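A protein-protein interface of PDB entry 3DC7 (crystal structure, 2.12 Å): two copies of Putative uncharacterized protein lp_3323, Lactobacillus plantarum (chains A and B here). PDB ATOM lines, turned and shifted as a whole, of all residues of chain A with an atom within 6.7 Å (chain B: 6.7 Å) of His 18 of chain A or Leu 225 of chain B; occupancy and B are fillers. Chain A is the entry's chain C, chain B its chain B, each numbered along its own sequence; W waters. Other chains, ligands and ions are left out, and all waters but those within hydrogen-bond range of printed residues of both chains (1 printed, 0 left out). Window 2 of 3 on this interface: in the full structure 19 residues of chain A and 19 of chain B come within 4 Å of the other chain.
O of His 223 of chain B lies within hydrogen-bond range of NZ of Lys 215 of chain A, 3.1 Å away.
A ring nitrogen (ND1) of His 223 of chain B is in hydrogen-bond range of the side-chain hydroxyl of Ser 222 of chain B (3.2 Å).
The side-chain carboxylate of Asp 221 of chain A sits close to a ring nitrogen (NE2) of His 18 of chain A, at 3.4 Å.
His 18 of chain A touches Leu 225 of chain B (NE2 to CD2, 3.9 Å).
CB of Leu 225 of chain B touches NH1 of Arg 214 of chain A, at 3.5 Å.
Arg 214 of chain A touches Glu 226 of chain B.
Lys 215 of chain A touches Phe 224 of chain B (NZ to CD1, 3.4 Å).
Ser 218 of chain A touches Ser 222 of chain B.
C of His 223 of chain B touches OG of Ser 218 of chain A, 3.7 Å away.
Phe 224 of chain B touches Ser 218 of chain A (N to OG, 3.9 Å).
Leu 225 of chain B touches Ser 218 of chain A.
Printed residues of chain B within 4 Å of His 18 of chain A: Leu 225.
Leu 225 of chain B touches just these residues of chain A: His 18, Arg 214 and Ser 218.
Of the printed residues of chain B, Arg 214 of chain A touches Leu 225 and Glu 226.
Of the printed residues of chain A, Glu 226 of chain B touches Arg 214.
The nearest residue of chain A that does not touch Leu 225 of chain B is Gln 217 of chain A (4.3 Å).
Of the 11 printed residues of chain A, 4 touch a printed residue of chain B.
Printed residues of chain A that touch a printed residue of chain B: His 18, Arg 214, Lys 215 and Ser 218.
Hydrophobic or aromatic side chains of chain A that line the printed part of chain B: His 18.
Of the 10 printed residues of chain B, 5 touch a printed residue of chain A.
Among the printed residues, no Asp or Glu carboxylate lies within 4 Å of a Lys or Arg side-chain nitrogen of the other chain.
3 positions are printed for both chains.
Of the 9 pairs that touch across the chains among the printed residues, none has its exchanged pair printed and touching as well.
Water W1 lies within hydrogen-bond range of the guanidinium group (NH1) of Arg 214 of chain A (3.2 Å) and the backbone NH (N) of Leu 225 of chain B (3.2 Å).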
ATOM      1  N   HIS A  18      20.784 -23.400  -5.297  1.00  0.00           N
ATOM      2  CA  HIS A  18      20.592 -22.743  -6.629  1.00  0.00           C
ATOM      3  C   HIS A  18      21.277 -23.475  -7.767  1.00  0.00           C
ATOM      4  O   HIS A  18      22.467 -23.748  -7.710  1.00  0.00           O
ATOM      5  CB  HIS A  18      21.116 -21.317  -6.601  1.00  0.00           C
ATOM      6  CG  HIS A  18      20.087 -20.298  -6.232  1.00  0.00           C
ATOM      7  ND1 HIS A  18      20.191 -19.513  -5.104  1.00  0.00           N
ATOM      8  CD2 HIS A  18      18.945 -19.918  -6.852  1.00  0.00           C
ATOM      9  CE1 HIS A  18      19.154 -18.695  -5.043  1.00  0.00           C
ATOM     10  NE2 HIS A  18      18.383 -18.922  -6.090  1.00  0.00           N
ATOM     11  N   VAL A  19      20.524 -23.761  -8.823  1.00  0.00           N
ATOM     12  CA  VAL A  19      21.095 -24.376 -10.016  1.00  0.00           C
ATOM     13  C   VAL A  19      22.022 -23.394 -10.746  1.00  0.00           C
ATOM     14  O   VAL A  19      21.713 -22.198 -10.880  1.00  0.00           O
ATOM     15  CB  VAL A  19      19.989 -24.882 -10.940  1.00  0.00           C
ATOM     16  CG1 VAL A  19      20.560 -25.452 -12.235  1.00  0.00           C
ATOM     17  CG2 VAL A  19      19.173 -25.925 -10.211  1.00  0.00           C
ATOM     18  N   SER A  20      23.173 -23.906 -11.174  1.00  0.00           N
ATOM     19  CA  SER A  20      24.125 -23.147 -11.958  1.00  0.00           C
ATOM     20  C   SER A  20      24.839 -24.053 -12.929  1.00  0.00           C
ATOM     21  O   SER A  20      24.891 -25.259 -12.743  1.00  0.00           O
ATOM     22  CB  SER A  20      25.145 -22.443 -11.062  1.00  0.00           C
ATOM     23  OG  SER A  20      26.103 -23.346 -10.554  1.00  0.00           O
ATOM     24  N   TRP A  50      26.712 -17.364 -11.541  1.00  0.00           N
ATOM     25  CA  TRP A  50      27.106 -18.766 -11.622  1.00  0.00           C
ATOM     26  C   TRP A  50      28.619 -18.927 -11.611  1.00  0.00           C
ATOM     27  O   TRP A  50      29.109 -20.045 -11.511  1.00  0.00           O
ATOM     28  CB  TRP A  50      26.555 -19.435 -12.891  1.00  0.00           C
ATOM     29  CG  TRP A  50      25.064 -19.541 -12.999  1.00  0.00           C
ATOM     30  CD1 TRP A  50      24.148 -19.387 -12.000  1.00  0.00           C
ATOM     31  CD2 TRP A  50      24.323 -19.895 -14.174  1.00  0.00           C
ATOM     32  NE1 TRP A  50      22.878 -19.595 -12.478  1.00  0.00           N
ATOM     33  CE2 TRP A  50      22.954 -19.912 -13.812  1.00  0.00           C
ATOM     34  CE3 TRP A  50      24.681 -20.197 -15.501  1.00  0.00           C
ATOM     35  CZ2 TRP A  50      21.946 -20.220 -14.720  1.00  0.00           C
ATOM     36  CZ3 TRP A  50      23.671 -20.496 -16.414  1.00  0.00           C
ATOM     37  CH2 TRP A  50      22.317 -20.505 -16.014  1.00  0.00           C
ATOM     38  N   ALA A 213      16.308 -12.701 -15.754  1.00  0.00           N
ATOM     39  CA  ALA A 213      17.283 -13.461 -14.964  1.00  0.00           C
ATOM     40  C   ALA A 213      16.670 -14.086 -13.715  1.00  0.00           C
ATOM     41  O   ALA A 213      16.997 -15.222 -13.382  1.00  0.00           O
ATOM     42  CB  ALA A 213      18.490 -12.575 -14.589  1.00  0.00           C
ATOM     43  N   ARG A 214      15.776 -13.357 -13.040  1.00  0.00           N
ATOM     44  CA  ARG A 214      15.096 -13.869 -11.851  1.00  0.00           C
ATOM     45  C   ARG A 214      14.156 -15.028 -12.187  1.00  0.00           C
ATOM     46  O   ARG A 214      14.173 -16.038 -11.515  1.00  0.00           O
ATOM     47  CB  ARG A 214      14.284 -12.781 -11.145  1.00  0.00           C
ATOM     48  CG  ARG A 214      15.091 -11.798 -10.310  1.00  0.00           C
ATOM     49  CD  ARG A 214      14.145 -10.782  -9.653  1.00  0.00           C
ATOM     50  NE  ARG A 214      14.669 -10.401  -8.357  1.00  0.00           N
ATOM     51  CZ  ARG A 214      14.204 -10.826  -7.187  1.00  0.00           C
ATOM     52  NH1 ARG A 214      13.146 -11.618  -7.120  1.00  0.00           N
ATOM     53  NH2 ARG A 214      14.793 -10.427  -6.074  1.00  0.00           N
ATOM     54  N   LYS A 215      13.353 -14.859 -13.229  1.00  0.00           N
ATOM     55  CA  LYS A 215      12.427 -15.879 -13.675  1.00  0.00           C
ATOM     56  C   LYS A 215      13.139 -17.127 -14.195  1.00  0.00           C
ATOM     57  O   LYS A 215      12.723 -18.244 -13.907  1.00  0.00           O
ATOM     58  CB  LYS A 215      11.500 -15.299 -14.743  1.00  0.00           C
ATOM     59  CG  LYS A 215      10.668 -14.139 -14.253  1.00  0.00           C
ATOM     60  CD  LYS A 215       9.725 -14.564 -13.125  1.00  0.00           C
ATOM     61  CE  LYS A 215       9.258 -13.360 -12.333  1.00  0.00           C
ATOM     62  NZ  LYS A 215       8.332 -13.753 -11.230  1.00  0.00           N
ATOM     63  N   GLN A 217      16.256 -18.127 -13.292  1.00  0.00           N
ATOM     64  CA  GLN A 217      16.842 -18.759 -12.114  1.00  0.00           C
ATOM     65  C   GLN A 217      15.826 -19.575 -11.305  1.00  0.00           C
ATOM     66  O   GLN A 217      16.148 -20.689 -10.883  1.00  0.00           O
ATOM     67  CB  GLN A 217      17.578 -17.755 -11.227  1.00  0.00           C
ATOM     68  CG  GLN A 217      18.378 -18.394 -10.089  1.00  0.00           C
ATOM     69  CD  GLN A 217      19.523 -19.281 -10.580  1.00  0.00           C
ATOM     70  OE1 GLN A 217      19.499 -20.500 -10.403  1.00  0.00           O
ATOM     71  NE2 GLN A 217      20.517 -18.674 -11.211  1.00  0.00           N
ATOM     72  N   SER A 218      14.615 -19.049 -11.086  1.00  0.00           N
ATOM     73  CA  SER A 218      13.635 -19.832 -10.320  1.00  0.00           C
ATOM     74  C   SER A 218      12.983 -20.958 -11.130  1.00  0.00           C
ATOM     75  O   SER A 218      12.575 -21.970 -10.553  1.00  0.00           O
ATOM     76  CB  SER A 218      12.600 -18.970  -9.617  1.00  0.00           C
ATOM     77  OG  SER A 218      11.546 -18.640 -10.478  1.00  0.00           O
ATOM     78  N   PHE A 219      12.908 -20.803 -12.456  1.00  0.00           N
ATOM     79  CA  PHE A 219      12.490 -21.898 -13.315  1.00  0.00           C
ATOM     80  C   PHE A 219      13.473 -23.066 -13.221  1.00  0.00           C
ATOM     81  O   PHE A 219      13.063 -24.219 -13.082  1.00  0.00           O
ATOM     82  CB  PHE A 219      12.397 -21.456 -14.771  1.00  0.00           C
ATOM     83  CG  PHE A 219      11.727 -22.462 -15.664  1.00  0.00           C
ATOM     84  CD1 PHE A 219      10.325 -22.551 -15.710  1.00  0.00           C
ATOM     85  CD2 PHE A 219      12.481 -23.317 -16.459  1.00  0.00           C
ATOM     86  CE1 PHE A 219       9.681 -23.469 -16.532  1.00  0.00           C
ATOM     87  CE2 PHE A 219      11.842 -24.251 -17.301  1.00  0.00           C
ATOM     88  CZ  PHE A 219      10.444 -24.322 -17.337  1.00  0.00           C
ATOM     89  N   ASP A 221      15.645 -23.725 -10.812  1.00  0.00           N
ATOM     90  CA  ASP A 221      15.498 -24.309  -9.474  1.00  0.00           C
ATOM     91  C   ASP A 221      14.341 -25.307  -9.364  1.00  0.00           C
ATOM     92  O   ASP A 221      14.438 -26.290  -8.623  1.00  0.00           O
ATOM     93  CB  ASP A 221      15.334 -23.211  -8.423  1.00  0.00           C
ATOM     94  CG  ASP A 221      16.625 -22.444  -8.161  1.00  0.00           C
ATOM     95  OD1 ASP A 221      17.660 -22.724  -8.817  1.00  0.00           O
ATOM     96  OD2 ASP A 221      16.602 -21.546  -7.288  1.00  0.00           O
ATOM     97  N   VAL B  19       9.455 -17.537  -0.222  1.00  0.00           N
ATOM     98  CA  VAL B  19       8.970 -16.243  -0.667  1.00  0.00           C
ATOM     99  C   VAL B  19       7.890 -15.744   0.294  1.00  0.00           C
ATOM    100  O   VAL B  19       6.928 -16.462   0.613  1.00  0.00           O
ATOM    101  CB  VAL B  19       8.392 -16.329  -2.084  1.00  0.00           C
ATOM    102  CG1 VAL B  19       7.947 -14.959  -2.568  1.00  0.00           C
ATOM    103  CG2 VAL B  19       9.410 -16.954  -3.039  1.00  0.00           C
ATOM    104  N   SER B  20       8.060 -14.509   0.749  1.00  0.00           N
ATOM    105  CA  SER B  20       7.106 -13.878   1.638  1.00  0.00           C
ATOM    106  C   SER B  20       6.950 -12.397   1.300  1.00  0.00           C
ATOM    107  O   SER B  20       7.789 -11.800   0.625  1.00  0.00           O
ATOM    108  CB  SER B  20       7.514 -14.079   3.097  1.00  0.00           C
ATOM    109  OG  SER B  20       8.681 -13.339   3.399  1.00  0.00           O
ATOM    110  N   PHE B  21       5.847 -11.818   1.737  1.00  0.00           N
ATOM    111  CA  PHE B  21       5.570 -10.438   1.432  1.00  0.00           C
ATOM    112  C   PHE B  21       5.104  -9.792   2.702  1.00  0.00           C
ATOM    113  O   PHE B  21       4.567 -10.474   3.573  1.00  0.00           O
ATOM    114  CB  PHE B  21       4.504 -10.328   0.335  1.00  0.00           C
ATOM    115  CG  PHE B  21       4.920 -10.947  -0.961  1.00  0.00           C
ATOM    116  CD1 PHE B  21       5.823 -10.294  -1.797  1.00  0.00           C
ATOM    117  CD2 PHE B  21       4.426 -12.197  -1.340  1.00  0.00           C
ATOM    118  CE1 PHE B  21       6.213 -10.864  -2.995  1.00  0.00           C
ATOM    119  CE2 PHE B  21       4.818 -12.781  -2.538  1.00  0.00           C
ATOM    120  CZ  PHE B  21       5.701 -12.116  -3.371  1.00  0.00           C
ATOM    121  N   LEU B 220       4.266 -19.971  -5.052  1.00  0.00           N
ATOM    122  CA  LEU B 220       5.096 -18.779  -4.867  1.00  0.00           C
ATOM    123  C   LEU B 220       6.602 -19.085  -4.893  1.00  0.00           C
ATOM    124  O   LEU B 220       7.368 -18.325  -5.468  1.00  0.00           O
ATOM    125  CB  LEU B 220       4.728 -18.058  -3.572  1.00  0.00           C
ATOM    126  CG  LEU B 220       3.933 -16.752  -3.591  1.00  0.00           C
ATOM    127  CD1 LEU B 220       3.156 -16.518  -4.867  1.00  0.00           C
ATOM    128  CD2 LEU B 220       3.032 -16.674  -2.388  1.00  0.00           C
ATOM    129  N   ASP B 221       7.011 -20.199  -4.286  1.00  0.00           N
ATOM    130  CA  ASP B 221       8.427 -20.594  -4.260  1.00  0.00           C
ATOM    131  C   ASP B 221       8.988 -21.046  -5.619  1.00  0.00           C
ATOM    132  O   ASP B 221      10.190 -20.980  -5.844  1.00  0.00           O
ATOM    133  CB  ASP B 221       8.668 -21.695  -3.221  1.00  0.00           C
ATOM    134  CG  ASP B 221       8.386 -21.241  -1.777  1.00  0.00           C
ATOM    135  OD1 ASP B 221       8.253 -20.019  -1.511  1.00  0.00           O
ATOM    136  OD2 ASP B 221       8.307 -22.137  -0.898  1.00  0.00           O
ATOM    137  N   SER B 222       8.129 -21.524  -6.512  1.00  0.00           N
ATOM    138  CA  SER B 222       8.587 -22.008  -7.814  1.00  0.00           C
ATOM    139  C   SER B 222       8.437 -20.982  -8.932  1.00  0.00           C
ATOM    140  O   SER B 222       8.955 -21.179 -10.031  1.00  0.00           O
ATOM    141  CB  SER B 222       7.902 -23.332  -8.190  1.00  0.00           C
ATOM    142  OG  SER B 222       6.487 -23.209  -8.195  1.00  0.00           O
ATOM    143  N   HIS B 223       7.764 -19.873  -8.651  1.00  0.00           N
ATOM    144  CA  HIS B 223       7.564 -18.841  -9.658  1.00  0.00           C
ATOM    145  C   HIS B 223       8.220 -17.520  -9.295  1.00  0.00           C
ATOM    146  O   HIS B 223       8.264 -16.599 -10.113  1.00  0.00           O
ATOM    147  CB  HIS B 223       6.064 -18.631  -9.913  1.00  0.00           C
ATOM    148  CG  HIS B 223       5.441 -19.735 -10.693  1.00  0.00           C
ATOM    149  ND1 HIS B 223       5.258 -20.999 -10.171  1.00  0.00           N
ATOM    150  CD2 HIS B 223       4.997 -19.784 -11.970  1.00  0.00           C
ATOM    151  CE1 HIS B 223       4.721 -21.778 -11.091  1.00  0.00           C
ATOM    152  NE2 HIS B 223       4.547 -21.064 -12.189  1.00  0.00           N
ATOM    153  N   PHE B 224       8.704 -17.414  -8.065  1.00  0.00           N
ATOM    154  CA  PHE B 224       9.301 -16.174  -7.598  1.00  0.00           C
ATOM    155  C   PHE B 224      10.614 -16.459  -6.886  1.00  0.00           C
ATOM    156  O   PHE B 224      10.803 -17.542  -6.336  1.00  0.00           O
ATOM    157  CB  PHE B 224       8.331 -15.419  -6.683  1.00  0.00           C
ATOM    158  CG  PHE B 224       7.127 -14.864  -7.399  1.00  0.00           C
ATOM    159  CD1 PHE B 224       7.185 -13.625  -8.027  1.00  0.00           C
ATOM    160  CD2 PHE B 224       5.936 -15.585  -7.453  1.00  0.00           C
ATOM    161  CE1 PHE B 224       6.077 -13.118  -8.697  1.00  0.00           C
ATOM    162  CE2 PHE B 224       4.819 -15.089  -8.122  1.00  0.00           C
ATOM    163  CZ  PHE B 224       4.888 -13.850  -8.739  1.00  0.00           C
ATOM    164  N   LEU B 225      11.527 -15.495  -6.929  1.00  0.00           N
ATOM    165  CA  LEU B 225      12.797 -15.620  -6.222  1.00  0.00           C
ATOM    166  C   LEU B 225      12.739 -14.949  -4.858  1.00  0.00           C
ATOM    167  O   LEU B 225      11.810 -14.194  -4.560  1.00  0.00           O
ATOM    168  CB  LEU B 225      13.945 -15.000  -7.023  1.00  0.00           C
ATOM    169  CG  LEU B 225      14.891 -15.791  -7.934  1.00  0.00           C
ATOM    170  CD1 LEU B 225      16.207 -15.048  -8.008  1.00  0.00           C
ATOM    171  CD2 LEU B 225      15.138 -17.225  -7.472  1.00  0.00           C
ATOM    172  N   GLU B 226      13.753 -15.237  -4.044  1.00  0.00           N
ATOM    173  CA  GLU B 226      14.066 -14.467  -2.839  1.00  0.00           C
ATOM    174  C   GLU B 226      13.025 -14.665  -1.747  1.00  0.00           C
ATOM    175  O   GLU B 226      13.127 -15.622  -0.978  1.00  0.00           O
ATOM    176  CB  GLU B 226      14.280 -12.980  -3.182  1.00  0.00           C
ATOM    177  CG  GLU B 226      14.630 -12.096  -1.999  1.00  0.00           C
ATOM    178  CD  GLU B 226      13.415 -11.386  -1.431  1.00  0.00           C
ATOM    179  OE1 GLU B 226      12.353 -11.419  -2.095  1.00  0.00           O
ATOM    180  OE2 GLU B 226      13.526 -10.790  -0.330  1.00  0.00           O
HETATM  181  O   HOH W   1      10.928 -13.027  -8.955  1.00  0.00           O
